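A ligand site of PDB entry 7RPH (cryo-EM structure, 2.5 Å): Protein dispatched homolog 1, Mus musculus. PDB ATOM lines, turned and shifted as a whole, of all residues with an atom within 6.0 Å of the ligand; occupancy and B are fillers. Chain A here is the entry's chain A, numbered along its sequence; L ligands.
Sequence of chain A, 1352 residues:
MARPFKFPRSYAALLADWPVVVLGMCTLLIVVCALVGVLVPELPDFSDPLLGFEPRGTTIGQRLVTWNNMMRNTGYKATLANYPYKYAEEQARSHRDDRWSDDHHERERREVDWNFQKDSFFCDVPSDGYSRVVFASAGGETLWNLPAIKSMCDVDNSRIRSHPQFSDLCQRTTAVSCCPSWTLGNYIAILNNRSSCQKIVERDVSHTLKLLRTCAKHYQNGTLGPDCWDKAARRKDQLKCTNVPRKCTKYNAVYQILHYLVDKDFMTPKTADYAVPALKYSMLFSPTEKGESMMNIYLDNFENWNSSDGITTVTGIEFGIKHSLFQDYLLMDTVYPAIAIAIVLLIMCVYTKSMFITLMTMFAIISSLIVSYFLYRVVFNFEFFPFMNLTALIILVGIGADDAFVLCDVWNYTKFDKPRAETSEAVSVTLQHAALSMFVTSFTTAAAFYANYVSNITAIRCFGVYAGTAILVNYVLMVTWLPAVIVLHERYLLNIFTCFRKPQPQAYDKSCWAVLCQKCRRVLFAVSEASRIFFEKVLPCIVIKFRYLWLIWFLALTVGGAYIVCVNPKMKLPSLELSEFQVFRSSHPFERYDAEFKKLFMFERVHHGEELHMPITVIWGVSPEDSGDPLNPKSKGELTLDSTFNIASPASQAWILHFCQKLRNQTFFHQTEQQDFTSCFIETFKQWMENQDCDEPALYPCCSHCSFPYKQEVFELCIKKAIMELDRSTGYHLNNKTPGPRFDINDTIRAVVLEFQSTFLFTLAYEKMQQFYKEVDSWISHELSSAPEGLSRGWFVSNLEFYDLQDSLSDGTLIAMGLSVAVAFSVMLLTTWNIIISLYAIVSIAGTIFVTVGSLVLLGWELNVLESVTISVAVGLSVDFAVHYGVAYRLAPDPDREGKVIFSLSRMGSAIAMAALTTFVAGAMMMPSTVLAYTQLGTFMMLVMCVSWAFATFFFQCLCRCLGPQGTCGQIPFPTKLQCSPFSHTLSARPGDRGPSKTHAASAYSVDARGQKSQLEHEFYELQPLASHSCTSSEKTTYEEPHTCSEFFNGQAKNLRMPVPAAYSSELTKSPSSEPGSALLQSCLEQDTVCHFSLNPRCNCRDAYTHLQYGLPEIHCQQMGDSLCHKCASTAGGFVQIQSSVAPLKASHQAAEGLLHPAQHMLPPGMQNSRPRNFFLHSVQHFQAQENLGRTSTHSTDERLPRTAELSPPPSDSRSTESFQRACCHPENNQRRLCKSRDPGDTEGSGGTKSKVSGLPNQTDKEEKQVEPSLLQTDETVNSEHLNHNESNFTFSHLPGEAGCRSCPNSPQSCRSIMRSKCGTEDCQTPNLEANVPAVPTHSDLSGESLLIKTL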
ATOM      1  N   ASN A 304      -2.939  -4.385  26.028  1.00  0.00           N
ATOM      2  CA  ASN A 304      -2.440  -3.130  26.621  1.00  0.00           C
ATOM      3  C   ASN A 304      -1.003  -3.246  27.163  1.00  0.00           C
ATOM      4  O   ASN A 304      -0.502  -2.322  27.806  1.00  0.00           O
ATOM      5  CB  ASN A 304      -3.462  -2.642  27.659  1.00  0.00           C
ATOM      6  CG  ASN A 304      -4.804  -2.361  26.993  1.00  0.00           C
ATOM      7  OD1 ASN A 304      -4.972  -1.368  26.298  1.00  0.00           O
ATOM      8  ND2 ASN A 304      -5.766  -3.246  27.133  1.00  0.00           N
ATOM      9  N   TYR A 329     -11.890  -2.653  17.811  1.00  0.00           N
ATOM     10  CA  TYR A 329     -11.038  -1.560  17.379  1.00  0.00           C
ATOM     11  C   TYR A 329     -11.754  -0.586  16.470  1.00  0.00           C
ATOM     12  O   TYR A 329     -11.621   0.615  16.644  1.00  0.00           O
ATOM     13  CB  TYR A 329      -9.800  -2.110  16.691  1.00  0.00           C
ATOM     14  CG  TYR A 329      -8.851  -2.851  17.602  1.00  0.00           C
ATOM     15  CD1 TYR A 329      -8.250  -2.167  18.672  1.00  0.00           C
ATOM     16  CD2 TYR A 329      -8.528  -4.186  17.363  1.00  0.00           C
ATOM     17  CE1 TYR A 329      -7.299  -2.813  19.471  1.00  0.00           C
ATOM     18  CE2 TYR A 329      -7.549  -4.826  18.139  1.00  0.00           C
ATOM     19  CZ  TYR A 329      -6.920  -4.135  19.187  1.00  0.00           C
ATOM     20  OH  TYR A 329      -5.922  -4.724  19.886  1.00  0.00           O
ATOM     21  N   LEU A 331     -14.983   0.237  16.372  1.00  0.00           N
ATOM     22  CA  LEU A 331     -15.880   1.064  17.152  1.00  0.00           C
ATOM     23  C   LEU A 331     -15.129   1.928  18.173  1.00  0.00           C
ATOM     24  O   LEU A 331     -15.486   3.087  18.345  1.00  0.00           O
ATOM     25  CB  LEU A 331     -16.976   0.195  17.760  1.00  0.00           C
ATOM     26  CG  LEU A 331     -17.865  -0.536  16.718  1.00  0.00           C
ATOM     27  CD1 LEU A 331     -18.841  -1.461  17.428  1.00  0.00           C
ATOM     28  CD2 LEU A 331     -18.692   0.395  15.840  1.00  0.00           C
ATOM     29  N   MET A 332     -14.039   1.466  18.793  1.00  0.00           N
ATOM     30  CA  MET A 332     -13.186   2.323  19.629  1.00  0.00           C
ATOM     31  C   MET A 332     -12.538   3.474  18.857  1.00  0.00           C
ATOM     32  O   MET A 332     -12.476   4.590  19.357  1.00  0.00           O
ATOM     33  CB  MET A 332     -12.040   1.508  20.237  1.00  0.00           C
ATOM     34  CG  MET A 332     -12.486   0.619  21.391  1.00  0.00           C
ATOM     35  SD  MET A 332     -11.512  -0.892  21.616  1.00  0.00           S
ATOM     36  CE  MET A 332      -9.828  -0.250  21.784  1.00  0.00           C
ATOM     37  N   ASP A 333     -12.028   3.239  17.662  1.00  0.00           N
ATOM     38  CA  ASP A 333     -11.336   4.244  16.875  1.00  0.00           C
ATOM     39  C   ASP A 333     -12.262   5.364  16.392  1.00  0.00           C
ATOM     40  O   ASP A 333     -11.777   6.378  15.916  1.00  0.00           O
ATOM     41  CB  ASP A 333     -10.570   3.598  15.706  1.00  0.00           C
ATOM     42  CG  ASP A 333      -9.263   2.871  16.054  1.00  0.00           C
ATOM     43  OD1 ASP A 333      -8.742   3.080  17.165  1.00  0.00           O
ATOM     44  OD2 ASP A 333      -8.690   2.185  15.192  1.00  0.00           O
ATOM     45  N   THR A 334     -13.585   5.275  16.575  1.00  0.00           N
ATOM     46  CA  THR A 334     -14.503   6.402  16.333  1.00  0.00           C
ATOM     47  C   THR A 334     -14.266   7.608  17.257  1.00  0.00           C
ATOM     48  O   THR A 334     -14.781   8.681  16.992  1.00  0.00           O
ATOM     49  CB  THR A 334     -15.977   6.003  16.438  1.00  0.00           C
ATOM     50  OG1 THR A 334     -16.292   5.572  17.734  1.00  0.00           O
ATOM     51  CG2 THR A 334     -16.357   4.903  15.458  1.00  0.00           C
ATOM     52  N   VAL A 335     -13.400   7.493  18.258  1.00  0.00           N
ATOM     53  CA  VAL A 335     -12.933   8.633  19.049  1.00  0.00           C
ATOM     54  C   VAL A 335     -12.134   9.660  18.244  1.00  0.00           C
ATOM     55  O   VAL A 335     -12.207  10.850  18.540  1.00  0.00           O
ATOM     56  CB  VAL A 335     -12.145   8.115  20.263  1.00  0.00           C
ATOM     57  CG1 VAL A 335     -10.761   7.562  19.912  1.00  0.00           C
ATOM     58  CG2 VAL A 335     -11.990   9.212  21.305  1.00  0.00           C
ATOM     59  N   TYR A 336     -11.389   9.285  17.206  1.00  0.00           N
ATOM     60  CA  TYR A 336     -10.611  10.254  16.419  1.00  0.00           C
ATOM     61  C   TYR A 336     -11.463  11.119  15.489  1.00  0.00           C
ATOM     62  O   TYR A 336     -11.252  12.327  15.487  1.00  0.00           O
ATOM     63  CB  TYR A 336      -9.430   9.609  15.705  1.00  0.00           C
ATOM     64  CG  TYR A 336      -8.607   8.685  16.563  1.00  0.00           C
ATOM     65  CD1 TYR A 336      -7.778   9.194  17.573  1.00  0.00           C
ATOM     66  CD2 TYR A 336      -8.726   7.299  16.380  1.00  0.00           C
ATOM     67  CE1 TYR A 336      -7.087   8.322  18.430  1.00  0.00           C
ATOM     68  CE2 TYR A 336      -8.054   6.423  17.250  1.00  0.00           C
ATOM     69  CZ  TYR A 336      -7.246   6.935  18.270  1.00  0.00           C
ATOM     70  OH  TYR A 336      -6.722   6.065  19.145  1.00  0.00           O
ATOM     71  N   PRO A 337     -12.477  10.604  14.771  1.00  0.00           N
ATOM     72  CA  PRO A 337     -13.465  11.428  14.074  1.00  0.00           C
ATOM     73  C   PRO A 337     -14.226  12.368  15.006  1.00  0.00           C
ATOM     74  O   PRO A 337     -14.553  13.477  14.607  1.00  0.00           O
ATOM     75  CB  PRO A 337     -14.424  10.449  13.398  1.00  0.00           C
ATOM     76  CG  PRO A 337     -13.593   9.188  13.227  1.00  0.00           C
ATOM     77  CD  PRO A 337     -12.699   9.212  14.453  1.00  0.00           C
ATOM     78  N   ALA A 338     -14.472  11.975  16.254  1.00  0.00           N
ATOM     79  CA  ALA A 338     -15.078  12.834  17.248  1.00  0.00           C
ATOM     80  C   ALA A 338     -14.172  14.008  17.631  1.00  0.00           C
ATOM     81  O   ALA A 338     -14.619  15.144  17.648  1.00  0.00           O
ATOM     82  CB  ALA A 338     -15.464  11.969  18.448  1.00  0.00           C
ATOM     83  N   ILE A 341     -14.195  16.629  14.690  1.00  0.00           N
ATOM     84  CA  ILE A 341     -15.354  17.516  14.820  1.00  0.00           C
ATOM     85  C   ILE A 341     -15.056  18.718  15.712  1.00  0.00           C
ATOM     86  O   ILE A 341     -15.323  19.834  15.299  1.00  0.00           O
ATOM     87  CB  ILE A 341     -16.595  16.734  15.283  1.00  0.00           C
ATOM     88  CG1 ILE A 341     -17.086  15.817  14.165  1.00  0.00           C
ATOM     89  CG2 ILE A 341     -17.743  17.637  15.733  1.00  0.00           C
ATOM     90  CD1 ILE A 341     -17.995  14.675  14.615  1.00  0.00           C
ATOM     91  N   ILE A 366     -23.719  16.294  10.385  1.00  0.00           N
ATOM     92  CA  ILE A 366     -24.031  15.002  11.006  1.00  0.00           C
ATOM     93  C   ILE A 366     -25.421  14.491  10.577  1.00  0.00           C
ATOM     94  O   ILE A 366     -25.586  13.318  10.260  1.00  0.00           O
ATOM     95  CB  ILE A 366     -23.869  15.129  12.536  1.00  0.00           C
ATOM     96  CG1 ILE A 366     -22.432  15.548  12.944  1.00  0.00           C
ATOM     97  CG2 ILE A 366     -24.245  13.826  13.243  1.00  0.00           C
ATOM     98  CD1 ILE A 366     -21.292  14.658  12.442  1.00  0.00           C
ATOM     99  N   LEU A 390     -18.518   3.407   7.419  1.00  0.00           N
ATOM    100  CA  LEU A 390     -18.147   4.217   8.586  1.00  0.00           C
ATOM    101  C   LEU A 390     -17.078   5.258   8.292  1.00  0.00           C
ATOM    102  O   LEU A 390     -17.050   6.283   8.935  1.00  0.00           O
ATOM    103  CB  LEU A 390     -17.629   3.329   9.716  1.00  0.00           C
ATOM    104  CG  LEU A 390     -18.675   2.452  10.393  1.00  0.00           C
ATOM    105  CD1 LEU A 390     -17.949   1.433  11.246  1.00  0.00           C
ATOM    106  CD2 LEU A 390     -19.576   3.261  11.307  1.00  0.00           C
ATOM    107  N   LEU A 393     -18.045   9.121   7.626  1.00  0.00           N
ATOM    108  CA  LEU A 393     -18.028  10.121   8.665  1.00  0.00           C
ATOM    109  C   LEU A 393     -16.790  11.016   8.592  1.00  0.00           C
ATOM    110  O   LEU A 393     -16.945  12.224   8.607  1.00  0.00           O
ATOM    111  CB  LEU A 393     -18.211   9.421  10.017  1.00  0.00           C
ATOM    112  CG  LEU A 393     -18.007  10.282  11.276  1.00  0.00           C
ATOM    113  CD1 LEU A 393     -18.972  11.452  11.394  1.00  0.00           C
ATOM    114  CD2 LEU A 393     -18.203   9.418  12.497  1.00  0.00           C
ATOM    115  N   PRO A 928      -3.335   8.518  14.523  1.00  0.00           N
ATOM    116  CA  PRO A 928      -3.192   7.628  15.670  1.00  0.00           C
ATOM    117  C   PRO A 928      -3.975   6.316  15.621  1.00  0.00           C
ATOM    118  O   PRO A 928      -3.765   5.469  16.468  1.00  0.00           O
ATOM    119  CB  PRO A 928      -3.582   8.463  16.890  1.00  0.00           C
ATOM    120  CG  PRO A 928      -4.417   9.569  16.303  1.00  0.00           C
ATOM    121  CD  PRO A 928      -3.756   9.825  14.992  1.00  0.00           C
ATOM    122  N   SER A 929      -4.858   6.091  14.650  1.00  0.00           N
ATOM    123  CA  SER A 929      -5.812   4.985  14.574  1.00  0.00           C
ATOM    124  C   SER A 929      -5.185   3.594  14.488  1.00  0.00           C
ATOM    125  O   SER A 929      -4.132   3.427  13.894  1.00  0.00           O
ATOM    126  CB  SER A 929      -6.692   5.265  13.382  1.00  0.00           C
ATOM    127  OG  SER A 929      -7.616   4.261  13.171  1.00  0.00           O
ATOM    128  N   THR A 930      -5.835   2.540  14.976  1.00  0.00           N
ATOM    129  CA  THR A 930      -5.406   1.149  14.789  1.00  0.00           C
ATOM    130  C   THR A 930      -5.926   0.554  13.513  1.00  0.00           C
ATOM    131  O   THR A 930      -5.218  -0.174  12.851  1.00  0.00           O
ATOM    132  CB  THR A 930      -5.856   0.237  15.936  1.00  0.00           C
ATOM    133  OG1 THR A 930      -5.498   0.794  17.144  1.00  0.00           O
ATOM    134  CG2 THR A 930      -5.199  -1.140  15.888  1.00  0.00           C
HETATM  135  C1  LIG L   1     -14.217   3.685  24.445  1.00  0.00           C
HETATM  136  O1  LIG L   1     -14.323   3.777  23.017  1.00  0.00           O
HETATM  137  C2  LIG L   1     -13.544   2.353  24.884  1.00  0.00           C
HETATM  138  O2  LIG L   1     -14.042   1.936  26.167  1.00  0.00           O
HETATM  139  C3  LIG L   1     -11.996   2.467  24.970  1.00  0.00           C
HETATM  140  O3  LIG L   1     -11.411   1.191  24.691  1.00  0.00           O
HETATM  141  C4  LIG L   1     -11.472   3.606  24.054  1.00  0.00           C
HETATM  142  O4  LIG L   1     -10.049   3.788  24.158  1.00  0.00           O
HETATM  143  C5  LIG L   1     -12.099   4.960  24.497  1.00  0.00           C
HETATM  144  O5  LIG L   1     -13.459   4.793  24.953  1.00  0.00           O
HETATM  145  C6  LIG L   1     -11.993   6.007  23.380  1.00  0.00           C
HETATM  146  O6  LIG L   1     -10.661   6.519  23.378  1.00  0.00           O
HETATM  147  C7  LIG L   1     -20.927   6.620  12.462  1.00  0.00           C
HETATM  148  C8  LIG L   1     -18.104  11.193  15.770  1.00  0.00           C
HETATM  149  O7  LIG L   1      -7.968   3.701  19.434  1.00  0.00           O
HETATM  150  O8  LIG L   1     -16.710  10.652  33.693  1.00  0.00           O
HETATM  151  O9  LIG L   1     -18.162   9.627  26.574  1.00  0.00           O
HETATM  152  O10 LIG L   1     -16.058   4.599  29.583  1.00  0.00           O
HETATM  153  O11 LIG L   1     -16.285   3.518  26.990  1.00  0.00           O
HETATM  154  O12 LIG L   1      -7.777   6.330  21.603  1.00  0.00           O
HETATM  155  O13 LIG L   1     -19.811   8.920  33.499  1.00  0.00           O
HETATM  156  O14 LIG L   1      -6.217   5.285  23.791  1.00  0.00           O
HETATM  157  O15 LIG L   1     -19.332   6.089  33.823  1.00  0.00           O
HETATM  158  O16 LIG L   1      -7.529   3.198  25.320  1.00  0.00           O
HETATM  159  O17 LIG L   1     -17.574   4.861  31.911  1.00  0.00           O
HETATM  160  C9  LIG L   1     -20.945   6.521  14.007  1.00  0.00           C
HETATM  161  C10 LIG L   1     -19.601  10.880  15.554  1.00  0.00           C
HETATM  162  C11 LIG L   1     -20.576   5.097  14.492  1.00  0.00           C
HETATM  163  C12 LIG L   1     -20.247  10.176  16.766  1.00  0.00           C
HETATM  164  C13 LIG L   1     -20.678   4.960  16.035  1.00  0.00           C
HETATM  165  C14 LIG L   1     -19.705   8.740  17.013  1.00  0.00           C
HETATM  166  C15 LIG L   1     -20.329   3.525  16.482  1.00  0.00           C
HETATM  167  C16 LIG L   1     -19.240   8.481  18.463  1.00  0.00           C
HETATM  168  C17 LIG L   1     -20.567   3.279  17.994  1.00  0.00           C
HETATM  169  C18 LIG L   1     -17.998   9.320  18.850  1.00  0.00           C
HETATM  170  C19 LIG L   1     -19.349   3.625  18.894  1.00  0.00           C
HETATM  171  C20 LIG L   1     -17.517   9.076  20.298  1.00  0.00           C
HETATM  172  C21 LIG L   1     -19.656   3.323  20.386  1.00  0.00           C
HETATM  173  C22 LIG L   1     -16.709   7.766  20.427  1.00  0.00           C
HETATM  174  C23 LIG L   1     -18.406   3.303  21.308  1.00  0.00           C
HETATM  175  C24 LIG L   1     -16.380   7.444  21.901  1.00  0.00           C
HETATM  176  C25 LIG L   1      -9.162   4.272  19.976  1.00  0.00           C
HETATM  177  C26 LIG L   1     -17.474  10.587  32.476  1.00  0.00           C
HETATM  178  C27 LIG L   1     -17.611   9.050  27.756  1.00  0.00           C
HETATM  179  C28 LIG L   1     -17.607   4.643  21.283  1.00  0.00           C
HETATM  180  C29 LIG L   1     -15.646   6.083  22.079  1.00  0.00           C
HETATM  181  C30 LIG L   1     -15.667   3.535  22.504  1.00  0.00           C
HETATM  182  C31 LIG L   1     -17.340   5.061  23.771  1.00  0.00           C
HETATM  183  O18 LIG L   1     -16.469   5.543  24.803  1.00  0.00           O
HETATM  184  O19 LIG L   1     -17.050   7.126  26.396  1.00  0.00           O
HETATM  185  O20 LIG L   1      -9.250   2.994  22.068  1.00  0.00           O
HETATM  186  O21 LIG L   1     -16.555   8.451  31.730  1.00  0.00           O
HETATM  187  O22 LIG L   1     -17.527   7.111  30.059  1.00  0.00           O
HETATM  188  C32 LIG L   1      -9.134   4.325  21.521  1.00  0.00           C
HETATM  189  C33 LIG L   1     -17.798   9.121  32.061  1.00  0.00           C
HETATM  190  C34 LIG L   1     -17.662   7.504  27.660  1.00  0.00           C
HETATM  191  C35 LIG L   1     -16.825   5.272  28.581  1.00  0.00           C
HETATM  192  C36 LIG L   1     -17.086   5.711  26.092  1.00  0.00           C
HETATM  193  C37 LIG L   1     -16.264   4.947  27.172  1.00  0.00           C
HETATM  194  C38 LIG L   1     -16.552   4.837  22.431  1.00  0.00           C
HETATM  195  C39 LIG L   1      -7.803   4.969  21.987  1.00  0.00           C
HETATM  196  C40 LIG L   1     -18.538   8.325  33.188  1.00  0.00           C
HETATM  197  C41 LIG L   1     -16.857   6.815  28.803  1.00  0.00           C
HETATM  198  C42 LIG L   1      -9.144   2.871  23.509  1.00  0.00           C
HETATM  199  C43 LIG L   1     -16.696   7.089  31.243  1.00  0.00           C
HETATM  200  C44 LIG L   1      -7.546   4.818  23.495  1.00  0.00           C
HETATM  201  C45 LIG L   1     -18.742   6.843  32.758  1.00  0.00           C
HETATM  202  C46 LIG L   1      -7.709   3.331  23.912  1.00  0.00           C
HETATM  203  C47 LIG L   1     -17.385   6.223  32.346  1.00  0.00           C
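The side-chain carboxylate of Asp 333 is in hydrogen-bond range of an oxygen (O7) of the ligand (2.5 Å).
OH of Tyr 336 is in hydrogen-bond range of O12 of the ligand (2.7 Å).
O3 of the ligand sits close to SD of Met 332, at 3.7 Å.
The side-chain carboxylate (OD2) of Asp 333 lies within hydrogen-bond range of the backbone NH (N) of Thr 930, at 2.9 Å.
OG of Ser 929 sits at hydrogen-bond distance from OD2 of Asp 333 (3.1 Å).
The side-chain hydroxyl (OG1) of Thr 334 is in hydrogen-bond range of the backbone carbonyl oxygen (O) of Leu 331.
Merely in contact with the ligand: Leu 331, Thr 334, Val 335, Ala 338, Ile 341, Leu 390 and Leu 393.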
